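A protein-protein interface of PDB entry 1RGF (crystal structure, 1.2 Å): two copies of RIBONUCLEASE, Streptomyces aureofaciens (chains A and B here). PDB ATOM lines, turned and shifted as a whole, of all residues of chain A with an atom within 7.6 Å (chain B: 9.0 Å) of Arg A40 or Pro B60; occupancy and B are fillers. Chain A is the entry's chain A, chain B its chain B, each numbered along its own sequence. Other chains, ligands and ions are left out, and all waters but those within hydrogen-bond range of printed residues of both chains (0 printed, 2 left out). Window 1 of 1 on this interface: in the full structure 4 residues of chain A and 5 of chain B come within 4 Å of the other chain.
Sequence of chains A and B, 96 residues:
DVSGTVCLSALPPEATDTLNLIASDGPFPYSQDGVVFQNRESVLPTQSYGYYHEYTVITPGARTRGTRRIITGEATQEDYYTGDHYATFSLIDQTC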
ATOM      1  N   PHE A  37      14.139   5.365  -1.062  1.00  0.00           N
ATOM      2  CA  PHE A  37      13.538   5.618   0.218  1.00  0.00           C
ATOM      3  C   PHE A  37      13.280   4.198   0.820  1.00  0.00           C
ATOM      4  O   PHE A  37      12.526   3.457   0.238  1.00  0.00           O
ATOM      5  CB  PHE A  37      12.295   6.421   0.137  1.00  0.00           C
ATOM      6  CG  PHE A  37      11.619   6.613   1.441  1.00  0.00           C
ATOM      7  CD1 PHE A  37      12.194   7.414   2.401  1.00  0.00           C
ATOM      8  CD2 PHE A  37      10.439   5.999   1.767  1.00  0.00           C
ATOM      9  CE1 PHE A  37      11.585   7.584   3.635  1.00  0.00           C
ATOM     10  CE2 PHE A  37       9.824   6.150   2.968  1.00  0.00           C
ATOM     11  CZ  PHE A  37      10.390   6.956   3.913  1.00  0.00           C
ATOM     12  N   GLN A  38      13.933   3.879   1.913  1.00  0.00           N
ATOM     13  CA  GLN A  38      13.778   2.528   2.466  1.00  0.00           C
ATOM     14  C   GLN A  38      12.483   2.200   3.181  1.00  0.00           C
ATOM     15  O   GLN A  38      12.229   0.983   3.357  1.00  0.00           O
ATOM     16  CB  GLN A  38      14.872   2.306   3.534  1.00  0.00           C
ATOM     17  CG  GLN A  38      16.230   1.935   3.111  1.00  0.00           C
ATOM     18  CD  GLN A  38      17.034   1.482   4.342  1.00  0.00           C
ATOM     19  OE1 GLN A  38      16.622   0.618   5.097  1.00  0.00           O
ATOM     20  NE2 GLN A  38      18.130   2.167   4.482  1.00  0.00           N
ATOM     21  N   ASN A  39      11.736   3.199   3.608  1.00  0.00           N
ATOM     22  CA  ASN A  39      10.501   2.964   4.340  1.00  0.00           C
ATOM     23  C   ASN A  39      10.809   2.045   5.543  1.00  0.00           C
ATOM     24  O   ASN A  39      10.016   1.156   5.883  1.00  0.00           O
ATOM     25  CB  ASN A  39       9.428   2.341   3.486  1.00  0.00           C
ATOM     26  CG  ASN A  39       8.054   2.321   4.022  1.00  0.00           C
ATOM     27  OD1 ASN A  39       7.659   3.236   4.724  1.00  0.00           O
ATOM     28  ND2 ASN A  39       7.304   1.229   3.713  1.00  0.00           N
ATOM     29  N   ARG A  40      11.875   2.341   6.257  1.00  0.00           N
ATOM     30  CA  ARG A  40      12.322   1.540   7.370  1.00  0.00           C
ATOM     31  C   ARG A  40      11.304   1.475   8.477  1.00  0.00           C
ATOM     32  O   ARG A  40      11.196   0.451   9.215  1.00  0.00           O
ATOM     33  CB  ARG A  40      13.662   2.096   7.834  1.00  0.00           C
ATOM     34  CG  ARG A  40      14.414   1.383   8.907  1.00  0.00           C
ATOM     35  CD  ARG A  40      15.950   1.384   8.658  1.00  0.00           C
ATOM     36  NE  ARG A  40      16.393   0.043   9.064  1.00  0.00           N
ATOM     37  CZ  ARG A  40      17.140  -0.949   8.639  1.00  0.00           C
ATOM     38  NH1 ARG A  40      17.779  -0.851   7.470  1.00  0.00           N
ATOM     39  NH2 ARG A  40      17.236  -2.040   9.415  1.00  0.00           N
ATOM     40  N   GLU A  41      10.513   2.531   8.691  1.00  0.00           N
ATOM     41  CA  GLU A  41       9.560   2.567   9.758  1.00  0.00           C
ATOM     42  C   GLU A  41       8.207   2.018   9.446  1.00  0.00           C
ATOM     43  O   GLU A  41       7.286   2.082  10.245  1.00  0.00           O
ATOM     44  CB  GLU A  41       9.380   4.004  10.304  1.00  0.00           C
ATOM     45  CG  GLU A  41      10.616   4.599  10.956  1.00  0.00           C
ATOM     46  CD  GLU A  41      11.803   4.933  10.057  1.00  0.00           C
ATOM     47  OE1 GLU A  41      11.706   5.583   8.960  1.00  0.00           O
ATOM     48  OE2 GLU A  41      12.884   4.469  10.545  1.00  0.00           O
ATOM     49  N   SER A  42       8.041   1.566   8.205  1.00  0.00           N
ATOM     50  CA  SER A  42       6.819   1.014   7.723  1.00  0.00           C
ATOM     51  C   SER A  42       5.622   1.933   7.760  1.00  0.00           C
ATOM     52  O   SER A  42       4.483   1.485   7.907  1.00  0.00           O
ATOM     53  CB  SER A  42       6.532  -0.298   8.518  1.00  0.00           C
ATOM     54  OG  SER A  42       5.616  -1.042   7.743  1.00  0.00           O
ATOM     55  N   VAL A  43       5.853   3.259   7.523  1.00  0.00           N
ATOM     56  CA  VAL A  43       4.773   4.193   7.440  1.00  0.00           C
ATOM     57  C   VAL A  43       3.975   4.069   6.145  1.00  0.00           C
ATOM     58  O   VAL A  43       2.765   4.138   6.094  1.00  0.00           O
ATOM     59  CB  VAL A  43       5.276   5.615   7.678  1.00  0.00           C
ATOM     60  CG1 VAL A  43       4.028   6.508   7.534  1.00  0.00           C
ATOM     61  CG2 VAL A  43       5.936   5.699   9.025  1.00  0.00           C
ATOM     62  N   LEU A  44       4.634   3.786   5.027  1.00  0.00           N
ATOM     63  CA  LEU A  44       4.014   3.546   3.784  1.00  0.00           C
ATOM     64  C   LEU A  44       3.825   2.028   3.603  1.00  0.00           C
ATOM     65  O   LEU A  44       4.481   1.232   4.259  1.00  0.00           O
ATOM     66  CB  LEU A  44       4.949   4.048   2.662  1.00  0.00           C
ATOM     67  CG  LEU A  44       5.160   5.581   2.644  1.00  0.00           C
ATOM     68  CD1 LEU A  44       6.041   5.984   1.503  1.00  0.00           C
ATOM     69  CD2 LEU A  44       3.869   6.325   2.544  1.00  0.00           C
ATOM     70  N   PRO B  12       2.134  -4.576  20.681  1.00  0.00           N
ATOM     71  CA  PRO B  12       2.527  -3.507  19.742  1.00  0.00           C
ATOM     72  C   PRO B  12       1.337  -3.190  18.929  1.00  0.00           C
ATOM     73  O   PRO B  12       0.436  -4.000  18.556  1.00  0.00           O
ATOM     74  CB  PRO B  12       3.651  -4.170  18.886  1.00  0.00           C
ATOM     75  CG  PRO B  12       4.199  -5.179  19.819  1.00  0.00           C
ATOM     76  CD  PRO B  12       2.983  -5.765  20.560  1.00  0.00           C
ATOM     77  N   PRO B  13       1.195  -1.937  18.462  1.00  0.00           N
ATOM     78  CA  PRO B  13       0.068  -1.507  17.677  1.00  0.00           C
ATOM     79  C   PRO B  13      -0.204  -2.269  16.399  1.00  0.00           C
ATOM     80  O   PRO B  13      -1.314  -2.412  15.890  1.00  0.00           O
ATOM     81  CB  PRO B  13       0.262   0.012  17.366  1.00  0.00           C
ATOM     82  CG  PRO B  13       1.635   0.253  17.894  1.00  0.00           C
ATOM     83  CD  PRO B  13       2.141  -0.850  18.755  1.00  0.00           C
ATOM     84  N   GLU B  14       0.864  -2.763  15.797  1.00  0.00           N
ATOM     85  CA  GLU B  14       0.815  -3.503  14.543  1.00  0.00           C
ATOM     86  C   GLU B  14       0.051  -4.833  14.687  1.00  0.00           C
ATOM     87  O   GLU B  14      -0.414  -5.398  13.696  1.00  0.00           O
ATOM     88  CB  GLU B  14       2.212  -3.743  13.978  1.00  0.00           C
ATOM     89  CG  GLU B  14       2.990  -2.479  13.602  1.00  0.00           C
ATOM     90  CD  GLU B  14       3.581  -1.754  14.782  1.00  0.00           C
ATOM     91  OE1 GLU B  14       3.793  -2.256  15.880  1.00  0.00           O
ATOM     92  OE2 GLU B  14       3.826  -0.515  14.554  1.00  0.00           O
ATOM     93  N   ALA B  15      -0.028  -5.318  15.918  1.00  0.00           N
ATOM     94  CA  ALA B  15      -0.824  -6.523  16.201  1.00  0.00           C
ATOM     95  C   ALA B  15      -2.269  -6.260  15.888  1.00  0.00           C
ATOM     96  O   ALA B  15      -3.002  -7.097  15.320  1.00  0.00           O
ATOM     97  CB  ALA B  15      -0.694  -6.975  17.632  1.00  0.00           C
ATOM     98  N   ASP B  17      -3.331  -4.053  13.616  1.00  0.00           N
ATOM     99  CA  ASP B  17      -3.367  -3.991  12.182  1.00  0.00           C
ATOM    100  C   ASP B  17      -3.544  -5.392  11.549  1.00  0.00           C
ATOM    101  O   ASP B  17      -4.364  -5.596  10.691  1.00  0.00           O
ATOM    102  CB  ASP B  17      -2.109  -3.359  11.582  1.00  0.00           C
ATOM    103  CG  ASP B  17      -1.899  -1.914  11.984  1.00  0.00           C
ATOM    104  OD1 ASP B  17      -2.918  -1.266  12.319  1.00  0.00           O
ATOM    105  OD2 ASP B  17      -0.713  -1.510  11.935  1.00  0.00           O
ATOM    106  N   TYR B  30       2.565  -9.549   2.880  1.00  0.00           N
ATOM    107  CA  TYR B  30       3.542 -10.532   2.536  1.00  0.00           C
ATOM    108  C   TYR B  30       2.936 -11.744   1.881  1.00  0.00           C
ATOM    109  O   TYR B  30       1.848 -12.153   2.308  1.00  0.00           O
ATOM    110  CB  TYR B  30       4.333 -10.969   3.748  1.00  0.00           C
ATOM    111  CG  TYR B  30       5.226  -9.868   4.243  1.00  0.00           C
ATOM    112  CD1 TYR B  30       6.404  -9.645   3.525  1.00  0.00           C
ATOM    113  CD2 TYR B  30       4.953  -9.082   5.319  1.00  0.00           C
ATOM    114  CE1 TYR B  30       7.322  -8.689   3.920  1.00  0.00           C
ATOM    115  CE2 TYR B  30       5.852  -8.083   5.734  1.00  0.00           C
ATOM    116  CZ  TYR B  30       7.010  -7.920   5.011  1.00  0.00           C
ATOM    117  OH  TYR B  30       7.928  -6.995   5.471  1.00  0.00           O
ATOM    118  N   VAL B  57       3.098  -9.840  11.914  1.00  0.00           N
ATOM    119  CA  VAL B  57       2.886  -8.622  12.688  1.00  0.00           C
ATOM    120  C   VAL B  57       4.213  -7.829  12.318  1.00  0.00           C
ATOM    121  O   VAL B  57       5.292  -8.215  12.656  1.00  0.00           O
ATOM    122  CB  VAL B  57       2.792  -8.796  14.193  1.00  0.00           C
ATOM    123  CG1 VAL B  57       2.765  -7.460  14.911  1.00  0.00           C
ATOM    124  CG2 VAL B  57       1.527  -9.583  14.508  1.00  0.00           C
ATOM    125  N   ILE B  58       3.999  -6.726  11.595  1.00  0.00           N
ATOM    126  CA  ILE B  58       5.168  -5.935  11.132  1.00  0.00           C
ATOM    127  C   ILE B  58       5.924  -5.353  12.297  1.00  0.00           C
ATOM    128  O   ILE B  58       5.306  -4.866  13.289  1.00  0.00           O
ATOM    129  CB  ILE B  58       4.684  -4.807  10.168  1.00  0.00           C
ATOM    130  CG1 ILE B  58       4.250  -5.466   8.875  1.00  0.00           C
ATOM    131  CG2 ILE B  58       5.843  -3.793   9.996  1.00  0.00           C
ATOM    132  CD1 ILE B  58       3.653  -4.547   7.853  1.00  0.00           C
ATOM    133  N   THR B  59       7.243  -5.375  12.270  1.00  0.00           N
ATOM    134  CA  THR B  59       8.085  -4.785  13.279  1.00  0.00           C
ATOM    135  C   THR B  59       8.756  -3.554  12.586  1.00  0.00           C
ATOM    136  O   THR B  59       9.609  -3.749  11.758  1.00  0.00           O
ATOM    137  CB  THR B  59       9.166  -5.728  13.728  1.00  0.00           C
ATOM    138  OG1 THR B  59       8.594  -6.907  14.357  1.00  0.00           O
ATOM    139  CG2 THR B  59      10.063  -5.064  14.756  1.00  0.00           C
ATOM    140  N   PRO B  60       8.307  -2.363  12.953  1.00  0.00           N
ATOM    141  CA  PRO B  60       8.909  -1.171  12.357  1.00  0.00           C
ATOM    142  C   PRO B  60      10.377  -1.162  12.671  1.00  0.00           C
ATOM    143  O   PRO B  60      10.799  -1.500  13.767  1.00  0.00           O
ATOM    144  CB  PRO B  60       8.235   0.020  13.047  1.00  0.00           C
ATOM    145  CG  PRO B  60       7.086  -0.574  13.757  1.00  0.00           C
ATOM    146  CD  PRO B  60       7.282  -2.062  13.934  1.00  0.00           C
ATOM    147  N   GLY B  61      11.244  -0.828  11.748  1.00  0.00           N
ATOM    148  CA  GLY B  61      12.668  -0.775  11.911  1.00  0.00           C
ATOM    149  C   GLY B  61      13.401  -2.041  11.576  1.00  0.00           C
ATOM    150  O   GLY B  61      14.626  -2.014  11.442  1.00  0.00           O
ATOM    151  N   ALA B  62      12.696  -3.188  11.433  1.00  0.00           N
ATOM    152  CA  ALA B  62      13.367  -4.420  11.128  1.00  0.00           C
ATOM    153  C   ALA B  62      13.638  -4.494   9.617  1.00  0.00           C
ATOM    154  O   ALA B  62      12.830  -3.979   8.860  1.00  0.00           O
ATOM    155  CB  ALA B  62      12.463  -5.576  11.508  1.00  0.00           C
ATOM    156  N   ARG B  63      14.703  -5.183   9.236  1.00  0.00           N
ATOM    157  CA  ARG B  63      14.991  -5.287   7.811  1.00  0.00           C
ATOM    158  C   ARG B  63      14.369  -6.485   7.149  1.00  0.00           C
ATOM    159  O   ARG B  63      14.394  -6.663   5.942  1.00  0.00           O
ATOM    160  CB  ARG B  63      16.485  -5.246   7.462  1.00  0.00           C
ATOM    161  CG  ARG B  63      17.349  -6.304   8.022  1.00  0.00           C
ATOM    162  CD  ARG B  63      18.730  -6.361   7.311  1.00  0.00           C
ATOM    163  NE  ARG B  63      18.502  -6.798   5.988  1.00  0.00           N
ATOM    164  CZ  ARG B  63      18.136  -7.893   5.375  1.00  0.00           C
ATOM    165  NH1 ARG B  63      17.955  -9.044   5.964  1.00  0.00           N
ATOM    166  NH2 ARG B  63      17.863  -7.724   4.098  1.00  0.00           N
ATOM    167  N   THR B  64      13.816  -7.369   7.995  1.00  0.00           N
ATOM    168  CA  THR B  64      13.147  -8.603   7.568  1.00  0.00           C
ATOM    169  C   THR B  64      11.701  -8.537   8.032  1.00  0.00           C
ATOM    170  O   THR B  64      11.280  -7.594   8.683  1.00  0.00           O
ATOM    171  CB  THR B  64      13.845  -9.817   8.196  1.00  0.00           C
ATOM    172  OG1 THR B  64      13.543  -9.875   9.599  1.00  0.00           O
ATOM    173  CG2 THR B  64      15.373  -9.902   8.071  1.00  0.00           C
ATOM    174  N   ARG B  65      10.995  -9.645   7.813  1.00  0.00           N
ATOM    175  CA  ARG B  65       9.653  -9.828   8.323  1.00  0.00           C
ATOM    176  C   ARG B  65       9.721  -9.945   9.872  1.00  0.00           C
ATOM    177  O   ARG B  65       8.619  -9.835  10.496  1.00  0.00           O
ATOM    178  CB  ARG B  65       8.913 -11.052   7.826  1.00  0.00           C
ATOM    179  CG  ARG B  65       8.267 -10.981   6.538  1.00  0.00           C
ATOM    180  CD  ARG B  65       7.201 -12.080   6.381  1.00  0.00           C
ATOM    181  NE  ARG B  65       7.577 -13.446   6.526  1.00  0.00           N
ATOM    182  CZ  ARG B  65       6.836 -14.417   7.048  1.00  0.00           C
ATOM    183  NH1 ARG B  65       5.646 -14.158   7.529  1.00  0.00           N
ATOM    184  NH2 ARG B  65       7.349 -15.655   7.015  1.00  0.00           N
ATOM    185  N   GLY B  66      10.859 -10.136  10.461  1.00  0.00           N
ATOM    186  CA  GLY B  66      10.935 -10.171  11.901  1.00  0.00           C
ATOM    187  C   GLY B  66      10.385 -11.470  12.523  1.00  0.00           C
ATOM    188  O   GLY B  66      10.252 -12.486  11.905  1.00  0.00           O
ATOM    189  N   ARG B  68       7.589 -11.425  14.983  1.00  0.00           N
ATOM    190  CA  ARG B  68       6.280 -11.274  15.518  1.00  0.00           C
ATOM    191  C   ARG B  68       5.243 -11.782  14.551  1.00  0.00           C
ATOM    192  O   ARG B  68       5.237 -11.468  13.368  1.00  0.00           O
ATOM    193  CB  ARG B  68       6.037  -9.819  15.898  1.00  0.00           C
ATOM    194  CG  ARG B  68       7.070  -9.215  16.765  1.00  0.00           C
ATOM    195  CD  ARG B  68       6.811  -7.738  17.034  1.00  0.00           C
ATOM    196  NE  ARG B  68       7.815  -7.291  18.004  1.00  0.00           N
ATOM    197  CZ  ARG B  68       7.929  -6.041  18.469  1.00  0.00           C
ATOM    198  NH1 ARG B  68       7.147  -5.100  18.034  1.00  0.00           N
ATOM    199  NH2 ARG B  68       8.860  -5.837  19.386  1.00  0.00           N
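N of Gly B61 sits at hydrogen-bond distance from O of Arg A40 (2.8 Å).
The side-chain amide oxygen of Gln A38 sits at hydrogen-bond distance from the guanidinium group of Arg A40 (3.0 Å).
Among the printed residues, merely in contact across the chains: Arg A40 with Pro B60 (3.9 Å), Arg A40 with Arg B63 (3.8 Å), Glu A41 with Pro B60 (3.6 Å) and Ser A42 with Ile B58 (3.6 Å).
Arg A40 touches just these residues of chain B: Pro B60, Gly B61 and Arg B63. Pro B60 touches just these residues of chain A: Arg A40 and Glu A41. Printed residues of chain A within 4 Å of Arg B63: Arg A40. Printed residues of chain B within 4 Å of Ser A42: Ile B58. Printed residues of chain A within 4 Å of Ile B58: Ser A42 (3.6 Å). Arg B65 touches none of the printed residues of chain A. The nearest residue of chain B that does not touch Arg A40 is Ala B62 (4.4 Å). The nearest printed residue of chain A that does not touch Pro B60 is Ser A42 (4.6 Å). The nearest printed residue of chain A that does not touch Ile B58 is Glu A41 (6.1 Å).
Among the printed residues, 5 pairs touch across the chains. Among the printed residues, no Asp or Glu carboxylate lies within 4 Å of a Lys or Arg side-chain nitrogen of the other chain.
No position is printed for both chains. Of the 5 pairs that touch across the chains among the printed residues, none has its exchanged pair printed and touching as well.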
